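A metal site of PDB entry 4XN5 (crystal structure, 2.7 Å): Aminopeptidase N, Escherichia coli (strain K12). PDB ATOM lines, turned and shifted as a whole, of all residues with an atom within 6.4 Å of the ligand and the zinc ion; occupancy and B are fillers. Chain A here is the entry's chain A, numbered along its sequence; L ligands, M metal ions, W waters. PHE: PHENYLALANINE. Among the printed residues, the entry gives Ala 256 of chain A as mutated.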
ATOM      1  N   GLN A 115      -8.389  30.915  -6.387  1.00  0.00           N
ATOM      2  CA  GLN A 115      -9.828  30.834  -6.445  1.00  0.00           C
ATOM      3  C   GLN A 115     -10.329  32.249  -6.607  1.00  0.00           C
ATOM      4  O   GLN A 115     -10.054  33.081  -5.721  1.00  0.00           O
ATOM      5  CB  GLN A 115     -10.406  30.203  -5.174  1.00  0.00           C
ATOM      6  CG  GLN A 115     -11.929  30.195  -5.146  1.00  0.00           C
ATOM      7  CD  GLN A 115     -12.548  29.579  -6.398  1.00  0.00           C
ATOM      8  OE1 GLN A 115     -11.990  28.639  -6.970  1.00  0.00           O
ATOM      9  NE2 GLN A 115     -13.713  30.102  -6.818  1.00  0.00           N
ATOM     10  N   GLU A 117     -13.722  33.142  -8.147  1.00  0.00           N
ATOM     11  CA  GLU A 117     -15.161  33.346  -7.939  1.00  0.00           C
ATOM     12  C   GLU A 117     -15.490  33.549  -6.450  1.00  0.00           C
ATOM     13  O   GLU A 117     -14.970  32.829  -5.598  1.00  0.00           O
ATOM     14  CB  GLU A 117     -16.017  32.214  -8.535  1.00  0.00           C
ATOM     15  CG  GLU A 117     -17.502  32.530  -8.561  1.00  0.00           C
ATOM     16  CD  GLU A 117     -18.407  31.488  -9.246  1.00  0.00           C
ATOM     17  OE1 GLU A 117     -17.967  30.452  -9.725  1.00  0.00           O
ATOM     18  OE2 GLU A 117     -19.622  31.724  -9.305  1.00  0.00           O
ATOM     19  N   ALA A 118     -16.332  34.523  -6.095  1.00  0.00           N
ATOM     20  CA  ALA A 118     -16.905  35.474  -7.033  1.00  0.00           C
ATOM     21  C   ALA A 118     -16.007  36.678  -7.238  1.00  0.00           C
ATOM     22  O   ALA A 118     -15.789  37.103  -8.375  1.00  0.00           O
ATOM     23  CB  ALA A 118     -18.301  35.922  -6.579  1.00  0.00           C
ATOM     24  N   TYR A 181     -13.445  36.231 -12.965  1.00  0.00           N
ATOM     25  CA  TYR A 181     -13.695  35.154 -11.998  1.00  0.00           C
ATOM     26  C   TYR A 181     -13.352  33.804 -12.540  1.00  0.00           C
ATOM     27  O   TYR A 181     -13.158  32.857 -11.771  1.00  0.00           O
ATOM     28  CB  TYR A 181     -15.141  35.143 -11.473  1.00  0.00           C
ATOM     29  CG  TYR A 181     -16.188  34.488 -12.346  1.00  0.00           C
ATOM     30  CD1 TYR A 181     -16.488  33.135 -12.201  1.00  0.00           C
ATOM     31  CD2 TYR A 181     -16.914  35.252 -13.252  1.00  0.00           C
ATOM     32  CE1 TYR A 181     -17.475  32.555 -12.993  1.00  0.00           C
ATOM     33  CE2 TYR A 181     -17.909  34.699 -14.029  1.00  0.00           C
ATOM     34  CZ  TYR A 181     -18.192  33.351 -13.915  1.00  0.00           C
ATOM     35  OH  TYR A 181     -19.137  32.828 -14.716  1.00  0.00           O
ATOM     36  N   PHE A 254      -9.204  23.904  -0.121  1.00  0.00           N
ATOM     37  CA  PHE A 254     -10.179  24.575  -0.948  1.00  0.00           C
ATOM     38  C   PHE A 254     -11.468  24.741  -0.155  1.00  0.00           C
ATOM     39  O   PHE A 254     -11.909  23.809   0.503  1.00  0.00           O
ATOM     40  CB  PHE A 254     -10.383  23.685  -2.170  1.00  0.00           C
ATOM     41  CG  PHE A 254     -10.991  24.374  -3.345  1.00  0.00           C
ATOM     42  CD1 PHE A 254     -10.227  25.153  -4.162  1.00  0.00           C
ATOM     43  CD2 PHE A 254     -12.306  24.177  -3.653  1.00  0.00           C
ATOM     44  CE1 PHE A 254     -10.764  25.785  -5.239  1.00  0.00           C
ATOM     45  CE2 PHE A 254     -12.871  24.815  -4.739  1.00  0.00           C
ATOM     46  CZ  PHE A 254     -12.094  25.626  -5.540  1.00  0.00           C
ATOM     47  N   ASN A 255     -12.085  25.929  -0.203  1.00  0.00           N
ATOM     48  CA  ASN A 255     -13.327  26.207   0.544  1.00  0.00           C
ATOM     49  C   ASN A 255     -14.613  25.552   0.034  1.00  0.00           C
ATOM     50  O   ASN A 255     -15.484  25.223   0.846  1.00  0.00           O
ATOM     51  CB  ASN A 255     -13.556  27.697   0.637  1.00  0.00           C
ATOM     52  CG  ASN A 255     -12.512  28.375   1.467  1.00  0.00           C
ATOM     53  OD1 ASN A 255     -11.866  27.726   2.301  1.00  0.00           O
ATOM     54  ND2 ASN A 255     -12.303  29.678   1.256  1.00  0.00           N
ATOM     55  N   ALA A 256     -14.748  25.358  -1.270  1.00  0.00           N
ATOM     56  CA  ALA A 256     -15.954  24.750  -1.853  1.00  0.00           C
ATOM     57  C   ALA A 256     -15.631  23.360  -2.451  1.00  0.00           C
ATOM     58  O   ALA A 256     -14.787  22.639  -1.905  1.00  0.00           O
ATOM     59  CB  ALA A 256     -16.575  25.701  -2.890  1.00  0.00           C
ATOM     60  N   GLY A 257     -16.307  22.989  -3.542  1.00  0.00           N
ATOM     61  CA  GLY A 257     -16.119  21.680  -4.152  1.00  0.00           C
ATOM     62  C   GLY A 257     -15.116  21.697  -5.295  1.00  0.00           C
ATOM     63  O   GLY A 257     -14.154  20.921  -5.309  1.00  0.00           O
ATOM     64  N   ALA A 258     -15.389  22.583  -6.247  1.00  0.00           N
ATOM     65  CA  ALA A 258     -14.632  22.731  -7.471  1.00  0.00           C
ATOM     66  C   ALA A 258     -15.026  24.050  -8.209  1.00  0.00           C
ATOM     67  O   ALA A 258     -16.090  24.643  -7.965  1.00  0.00           O
ATOM     68  CB  ALA A 258     -14.852  21.511  -8.347  1.00  0.00           C
ATOM     69  N   MET A 259     -14.137  24.508  -9.097  1.00  0.00           N
ATOM     70  CA  MET A 259     -14.318  25.756  -9.796  1.00  0.00           C
ATOM     71  C   MET A 259     -14.160  25.549 -11.312  1.00  0.00           C
ATOM     72  O   MET A 259     -13.148  24.953 -11.775  1.00  0.00           O
ATOM     73  CB  MET A 259     -13.285  26.736  -9.264  1.00  0.00           C
ATOM     74  CG  MET A 259     -13.405  28.116  -9.837  1.00  0.00           C
ATOM     75  SD  MET A 259     -15.078  28.765  -9.683  1.00  0.00           S
ATOM     76  CE  MET A 259     -15.277  29.643 -11.241  1.00  0.00           C
ATOM     77  N   GLU A 260     -15.106  26.088 -12.085  1.00  0.00           N
ATOM     78  CA  GLU A 260     -15.171  25.823 -13.525  1.00  0.00           C
ATOM     79  C   GLU A 260     -14.206  26.645 -14.375  1.00  0.00           C
ATOM     80  O   GLU A 260     -14.521  26.979 -15.503  1.00  0.00           O
ATOM     81  CB  GLU A 260     -16.617  25.994 -14.027  1.00  0.00           C
ATOM     82  CG  GLU A 260     -17.189  27.426 -13.986  1.00  0.00           C
ATOM     83  CD  GLU A 260     -17.928  27.753 -12.708  1.00  0.00           C
ATOM     84  OE1 GLU A 260     -17.701  27.105 -11.623  1.00  0.00           O
ATOM     85  OE2 GLU A 260     -18.763  28.676 -12.769  1.00  0.00           O
ATOM     86  N   VAL A 290     -19.704  16.166  -9.789  1.00  0.00           N
ATOM     87  CA  VAL A 290     -18.983  17.417  -9.740  1.00  0.00           C
ATOM     88  C   VAL A 290     -18.116  17.655 -11.007  1.00  0.00           C
ATOM     89  O   VAL A 290     -18.075  18.775 -11.580  1.00  0.00           O
ATOM     90  CB  VAL A 290     -18.191  17.516  -8.425  1.00  0.00           C
ATOM     91  CG1 VAL A 290     -17.408  18.833  -8.318  1.00  0.00           C
ATOM     92  CG2 VAL A 290     -19.144  17.434  -7.251  1.00  0.00           C
ATOM     93  N   HIS A 293     -20.589  18.589 -13.504  1.00  0.00           N
ATOM     94  CA  HIS A 293     -21.056  19.935 -13.169  1.00  0.00           C
ATOM     95  C   HIS A 293     -20.047  20.951 -13.652  1.00  0.00           C
ATOM     96  O   HIS A 293     -20.417  21.869 -14.400  1.00  0.00           O
ATOM     97  CB  HIS A 293     -21.220  20.059 -11.650  1.00  0.00           C
ATOM     98  CG  HIS A 293     -21.757  21.376 -11.191  1.00  0.00           C
ATOM     99  ND1 HIS A 293     -23.109  21.604 -10.981  1.00  0.00           N
ATOM    100  CD2 HIS A 293     -21.128  22.534 -10.884  1.00  0.00           C
ATOM    101  CE1 HIS A 293     -23.287  22.858 -10.599  1.00  0.00           C
ATOM    102  NE2 HIS A 293     -22.101  23.449 -10.542  1.00  0.00           N
ATOM    103  N   GLU A 294     -18.788  20.799 -13.247  1.00  0.00           N
ATOM    104  CA  GLU A 294     -17.817  21.797 -13.699  1.00  0.00           C
ATOM    105  C   GLU A 294     -17.668  21.711 -15.211  1.00  0.00           C
ATOM    106  O   GLU A 294     -17.498  22.724 -15.859  1.00  0.00           O
ATOM    107  CB  GLU A 294     -16.445  21.656 -13.060  1.00  0.00           C
ATOM    108  CG  GLU A 294     -16.424  21.636 -11.542  1.00  0.00           C
ATOM    109  CD  GLU A 294     -17.361  22.624 -10.873  1.00  0.00           C
ATOM    110  OE1 GLU A 294     -17.569  23.769 -11.323  1.00  0.00           O
ATOM    111  OE2 GLU A 294     -17.892  22.241  -9.849  1.00  0.00           O
ATOM    112  N   HIS A 297     -20.528  23.517 -16.931  1.00  0.00           N
ATOM    113  CA  HIS A 297     -20.341  24.976 -16.809  1.00  0.00           C
ATOM    114  C   HIS A 297     -19.625  25.582 -18.014  1.00  0.00           C
ATOM    115  O   HIS A 297     -19.655  26.817 -18.207  1.00  0.00           O
ATOM    116  CB  HIS A 297     -19.553  25.371 -15.528  1.00  0.00           C
ATOM    117  CG  HIS A 297     -20.422  25.790 -14.386  1.00  0.00           C
ATOM    118  ND1 HIS A 297     -21.459  26.678 -14.526  1.00  0.00           N
ATOM    119  CD2 HIS A 297     -20.395  25.440 -13.070  1.00  0.00           C
ATOM    120  CE1 HIS A 297     -22.043  26.854 -13.357  1.00  0.00           C
ATOM    121  NE2 HIS A 297     -21.428  26.105 -12.463  1.00  0.00           N
ATOM    122  N   LEU A 312     -26.603  34.792 -10.400  1.00  0.00           N
ATOM    123  CA  LEU A 312     -25.877  33.531 -10.227  1.00  0.00           C
ATOM    124  C   LEU A 312     -26.644  32.282 -10.689  1.00  0.00           C
ATOM    125  O   LEU A 312     -26.035  31.393 -11.319  1.00  0.00           O
ATOM    126  CB  LEU A 312     -25.445  33.336  -8.789  1.00  0.00           C
ATOM    127  CG  LEU A 312     -24.610  32.117  -8.402  1.00  0.00           C
ATOM    128  CD1 LEU A 312     -23.250  32.165  -9.064  1.00  0.00           C
ATOM    129  CD2 LEU A 312     -24.430  32.122  -6.896  1.00  0.00           C
ATOM    130  N   LYS A 315     -26.551  30.397 -14.171  1.00  0.00           N
ATOM    131  CA  LYS A 315     -25.598  29.333 -14.447  1.00  0.00           C
ATOM    132  C   LYS A 315     -25.639  28.161 -13.415  1.00  0.00           C
ATOM    133  O   LYS A 315     -25.393  27.025 -13.754  1.00  0.00           O
ATOM    134  CB  LYS A 315     -24.186  29.908 -14.557  1.00  0.00           C
ATOM    135  CG  LYS A 315     -23.520  30.210 -13.214  1.00  0.00           C
ATOM    136  CD  LYS A 315     -22.445  31.251 -13.328  1.00  0.00           C
ATOM    137  CE  LYS A 315     -21.101  30.764 -12.874  1.00  0.00           C
ATOM    138  NZ  LYS A 315     -20.856  30.670 -11.411  1.00  0.00           N
ATOM    139  N   GLU A 316     -25.905  28.471 -12.170  1.00  0.00           N
ATOM    140  CA  GLU A 316     -25.985  27.439 -11.187  1.00  0.00           C
ATOM    141  C   GLU A 316     -27.289  26.607 -11.230  1.00  0.00           C
ATOM    142  O   GLU A 316     -27.216  25.392 -11.237  1.00  0.00           O
ATOM    143  CB  GLU A 316     -25.759  28.015  -9.785  1.00  0.00           C
ATOM    144  CG  GLU A 316     -24.399  28.674  -9.603  1.00  0.00           C
ATOM    145  CD  GLU A 316     -23.276  27.754  -9.985  1.00  0.00           C
ATOM    146  OE1 GLU A 316     -23.518  26.540 -10.104  1.00  0.00           O
ATOM    147  OE2 GLU A 316     -22.145  28.244 -10.213  1.00  0.00           O
ATOM    148  N   THR A 319     -26.877  24.721 -14.457  1.00  0.00           N
ATOM    149  CA  THR A 319     -25.784  23.761 -14.457  1.00  0.00           C
ATOM    150  C   THR A 319     -26.019  22.613 -13.464  1.00  0.00           C
ATOM    151  O   THR A 319     -25.737  21.451 -13.786  1.00  0.00           O
ATOM    152  CB  THR A 319     -24.416  24.461 -14.267  1.00  0.00           C
ATOM    153  OG1 THR A 319     -24.180  25.393 -15.360  1.00  0.00           O
ATOM    154  CG2 THR A 319     -23.294  23.430 -14.213  1.00  0.00           C
ATOM    155  N   VAL A 320     -26.602  22.901 -12.296  1.00  0.00           N
ATOM    156  CA  VAL A 320     -27.099  21.823 -11.419  1.00  0.00           C
ATOM    157  C   VAL A 320     -28.144  20.934 -12.124  1.00  0.00           C
ATOM    158  O   VAL A 320     -28.041  19.700 -12.079  1.00  0.00           O
ATOM    159  CB  VAL A 320     -27.703  22.362 -10.108  1.00  0.00           C
ATOM    160  CG1 VAL A 320     -28.386  21.262  -9.318  1.00  0.00           C
ATOM    161  CG2 VAL A 320     -26.637  22.978  -9.211  1.00  0.00           C
ATOM    162  N   ASN A 369     -20.421  35.658  -1.346  1.00  0.00           N
ATOM    163  CA  ASN A 369     -20.175  34.238  -1.081  1.00  0.00           C
ATOM    164  C   ASN A 369     -21.220  33.618  -0.248  1.00  0.00           C
ATOM    165  O   ASN A 369     -21.360  32.383  -0.283  1.00  0.00           O
ATOM    166  CB  ASN A 369     -18.867  33.952  -0.398  1.00  0.00           C
ATOM    167  CG  ASN A 369     -17.686  34.093  -1.340  1.00  0.00           C
ATOM    168  OD1 ASN A 369     -16.701  34.743  -0.960  1.00  0.00           O
ATOM    169  ND2 ASN A 369     -17.772  33.536  -2.566  1.00  0.00           N
ATOM    170  N   TYR A 372     -24.090  31.451  -2.442  1.00  0.00           N
ATOM    171  CA  TYR A 372     -23.831  30.185  -3.076  1.00  0.00           C
ATOM    172  C   TYR A 372     -24.621  29.130  -2.278  1.00  0.00           C
ATOM    173  O   TYR A 372     -24.073  28.304  -1.596  1.00  0.00           O
ATOM    174  CB  TYR A 372     -22.314  29.963  -3.156  1.00  0.00           C
ATOM    175  CG  TYR A 372     -21.714  30.858  -4.238  1.00  0.00           C
ATOM    176  CD1 TYR A 372     -21.440  32.211  -4.002  1.00  0.00           C
ATOM    177  CD2 TYR A 372     -21.497  30.360  -5.514  1.00  0.00           C
ATOM    178  CE1 TYR A 372     -20.963  33.041  -5.012  1.00  0.00           C
ATOM    179  CE2 TYR A 372     -21.018  31.182  -6.547  1.00  0.00           C
ATOM    180  CZ  TYR A 372     -20.756  32.522  -6.294  1.00  0.00           C
ATOM    181  OH  TYR A 372     -20.305  33.318  -7.303  1.00  0.00           O
ATOM    182  N   TYR A 377     -28.799  27.213  -5.968  1.00  0.00           N
ATOM    183  CA  TYR A 377     -28.351  25.992  -6.685  1.00  0.00           C
ATOM    184  C   TYR A 377     -29.558  25.036  -6.919  1.00  0.00           C
ATOM    185  O   TYR A 377     -30.044  24.846  -8.017  1.00  0.00           O
ATOM    186  CB  TYR A 377     -27.213  25.289  -5.905  1.00  0.00           C
ATOM    187  CG  TYR A 377     -25.793  25.814  -6.153  1.00  0.00           C
ATOM    188  CD1 TYR A 377     -25.410  27.072  -5.780  1.00  0.00           C
ATOM    189  CD2 TYR A 377     -24.868  25.021  -6.751  1.00  0.00           C
ATOM    190  CE1 TYR A 377     -24.117  27.536  -6.010  1.00  0.00           C
ATOM    191  CE2 TYR A 377     -23.564  25.448  -6.996  1.00  0.00           C
ATOM    192  CZ  TYR A 377     -23.180  26.727  -6.636  1.00  0.00           C
ATOM    193  OH  TYR A 377     -21.852  27.148  -6.904  1.00  0.00           O
ATOM    194  N   GLN A 817     -15.224  32.623   4.792  1.00  0.00           N
ATOM    195  CA  GLN A 817     -16.115  31.731   4.032  1.00  0.00           C
ATOM    196  C   GLN A 817     -16.439  30.417   4.736  1.00  0.00           C
ATOM    197  O   GLN A 817     -17.593  30.000   4.740  1.00  0.00           O
ATOM    198  CB  GLN A 817     -15.545  31.392   2.682  1.00  0.00           C
ATOM    199  CG  GLN A 817     -15.332  32.620   1.811  1.00  0.00           C
ATOM    200  CD  GLN A 817     -15.000  32.241   0.377  1.00  0.00           C
ATOM    201  OE1 GLN A 817     -15.086  31.088   0.002  1.00  0.00           O
ATOM    202  NE2 GLN A 817     -14.651  33.221  -0.426  1.00  0.00           N
HETATM  203  N   PHE L   1     -18.637  27.936  -9.391  1.00  0.00           N
HETATM  204  CA  PHE L   1     -18.390  26.691  -8.580  1.00  0.00           C
HETATM  205  C   PHE L   1     -19.411  25.651  -8.973  1.00  0.00           C
HETATM  206  O   PHE L   1     -19.094  24.479  -9.067  1.00  0.00           O
HETATM  207  CB  PHE L   1     -18.585  26.839  -7.045  1.00  0.00           C
HETATM  208  CG  PHE L   1     -17.668  27.831  -6.333  1.00  0.00           C
HETATM  209  CD1 PHE L   1     -18.084  29.138  -6.068  1.00  0.00           C
HETATM  210  CD2 PHE L   1     -16.458  27.419  -5.802  1.00  0.00           C
HETATM  211  CE1 PHE L   1     -17.312  30.036  -5.339  1.00  0.00           C
HETATM  212  CE2 PHE L   1     -15.673  28.318  -5.069  1.00  0.00           C
HETATM  213  CZ  PHE L   1     -16.112  29.635  -4.848  1.00  0.00           C
HETATM  214  OXT PHE L   1     -20.593  25.996  -9.060  1.00  0.00           O
HETATM  215 ZN    ZN M   1     -21.739  25.551 -10.398  1.00  0.00          ZN
HETATM  216  O   HOH W   1     -20.121  26.500  -4.153  1.00  0.00           O
HETATM  217  O   HOH W   2     -18.900  24.285  -5.369  1.00  0.00           O
HETATM  218  O   HOH W   3     -13.231  27.706  -2.904  1.00  0.00           O
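Tyr 377 touches the zinc ion.
Four residues have an atom within 4 Å of the zinc ion: His 293, His 297, Glu 316 and Tyr 377.
The nearest printed residue that does not touch the zinc ion is Glu 260 (4.5 Å).
The side-chain carboxylate (OE1) of Glu 260 lies within salt-bridge range of a nitrogen (N) of the ligand (2.6 Å).
OE1 of Glu 117 lies within salt-bridge range of N of the ligand, 2.6 Å away.
SD of Met 259 is in hydrogen-bond range of N of the ligand, at 3.7 Å.
An oxygen (O) of the ligand sits close to the side-chain carboxylate (OE2) of Glu 294.
The side-chain hydroxyl (OH) of Tyr 377 lies close to an oxygen (OXT) of the ligand (2.7 Å).
An oxygen (OXT) of the ligand binds the zinc ion.
The side-chain carboxylate (OE1) of Glu 316 binds the zinc ion, 2.1 Å away.
NE2 of His 293 binds the zinc ion (2.1 Å).
NE2 of His 297 is bound to the zinc ion (2.2 Å).
Slightly farther from the zinc ion lies the side-chain carboxylate (OE2) of Glu 316 (2.7 Å).
The backbone carbonyl oxygen (O) of Ala 258 sits close to an oxygen (O) of the ligand (3.2 Å).
Merely in contact with the ligand: Gln 115, Ala 256 and Tyr 372.
Hydrophobic or aromatic side chains that line the ligand: Ala 256, Met 259, His 293, Tyr 372 and Tyr 377.
12 residues have an atom within 4 Å of the ligand: Gln 115, Glu 117, Ala 256, Ala 258, Met 259, Glu 260, His 293, Glu 294, His 297, Glu 316, Tyr 372 and Tyr 377.
OE2 of Glu 117 sits at hydrogen-bond distance from OH of Tyr 372, 2.6 Å away.
A ring nitrogen (ND1) of His 297 is in hydrogen-bond range of the side-chain hydroxyl (OG1) of Thr 319, at 3.1 Å.
The side-chain carboxylate (OE2) of Glu 260 lies within salt-bridge range of the side-chain amino group (NZ) of Lys 315 (3.2 Å).
OE2 of Glu 316 lies close to OH of Tyr 377 (3.5 Å).
The side-chain amide nitrogen (NE2) of Gln 115 sits at hydrogen-bond distance from the side-chain sulfur (SD) of Met 259, at 3.4 Å.
The side-chain carboxylate (OE2) of Glu 117 is in salt-bridge range of the side-chain amino group (NZ) of Lys 315, at 2.7 Å.
The backbone NH (N) of Glu 260 is in hydrogen-bond range of the side-chain carboxylate (OE1) of Glu 294, at 3.5 Å.
The side-chain carboxylate (OE2) of Glu 316 lies within salt-bridge range of the side-chain amino group (NZ) of Lys 315, at 3.0 Å.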
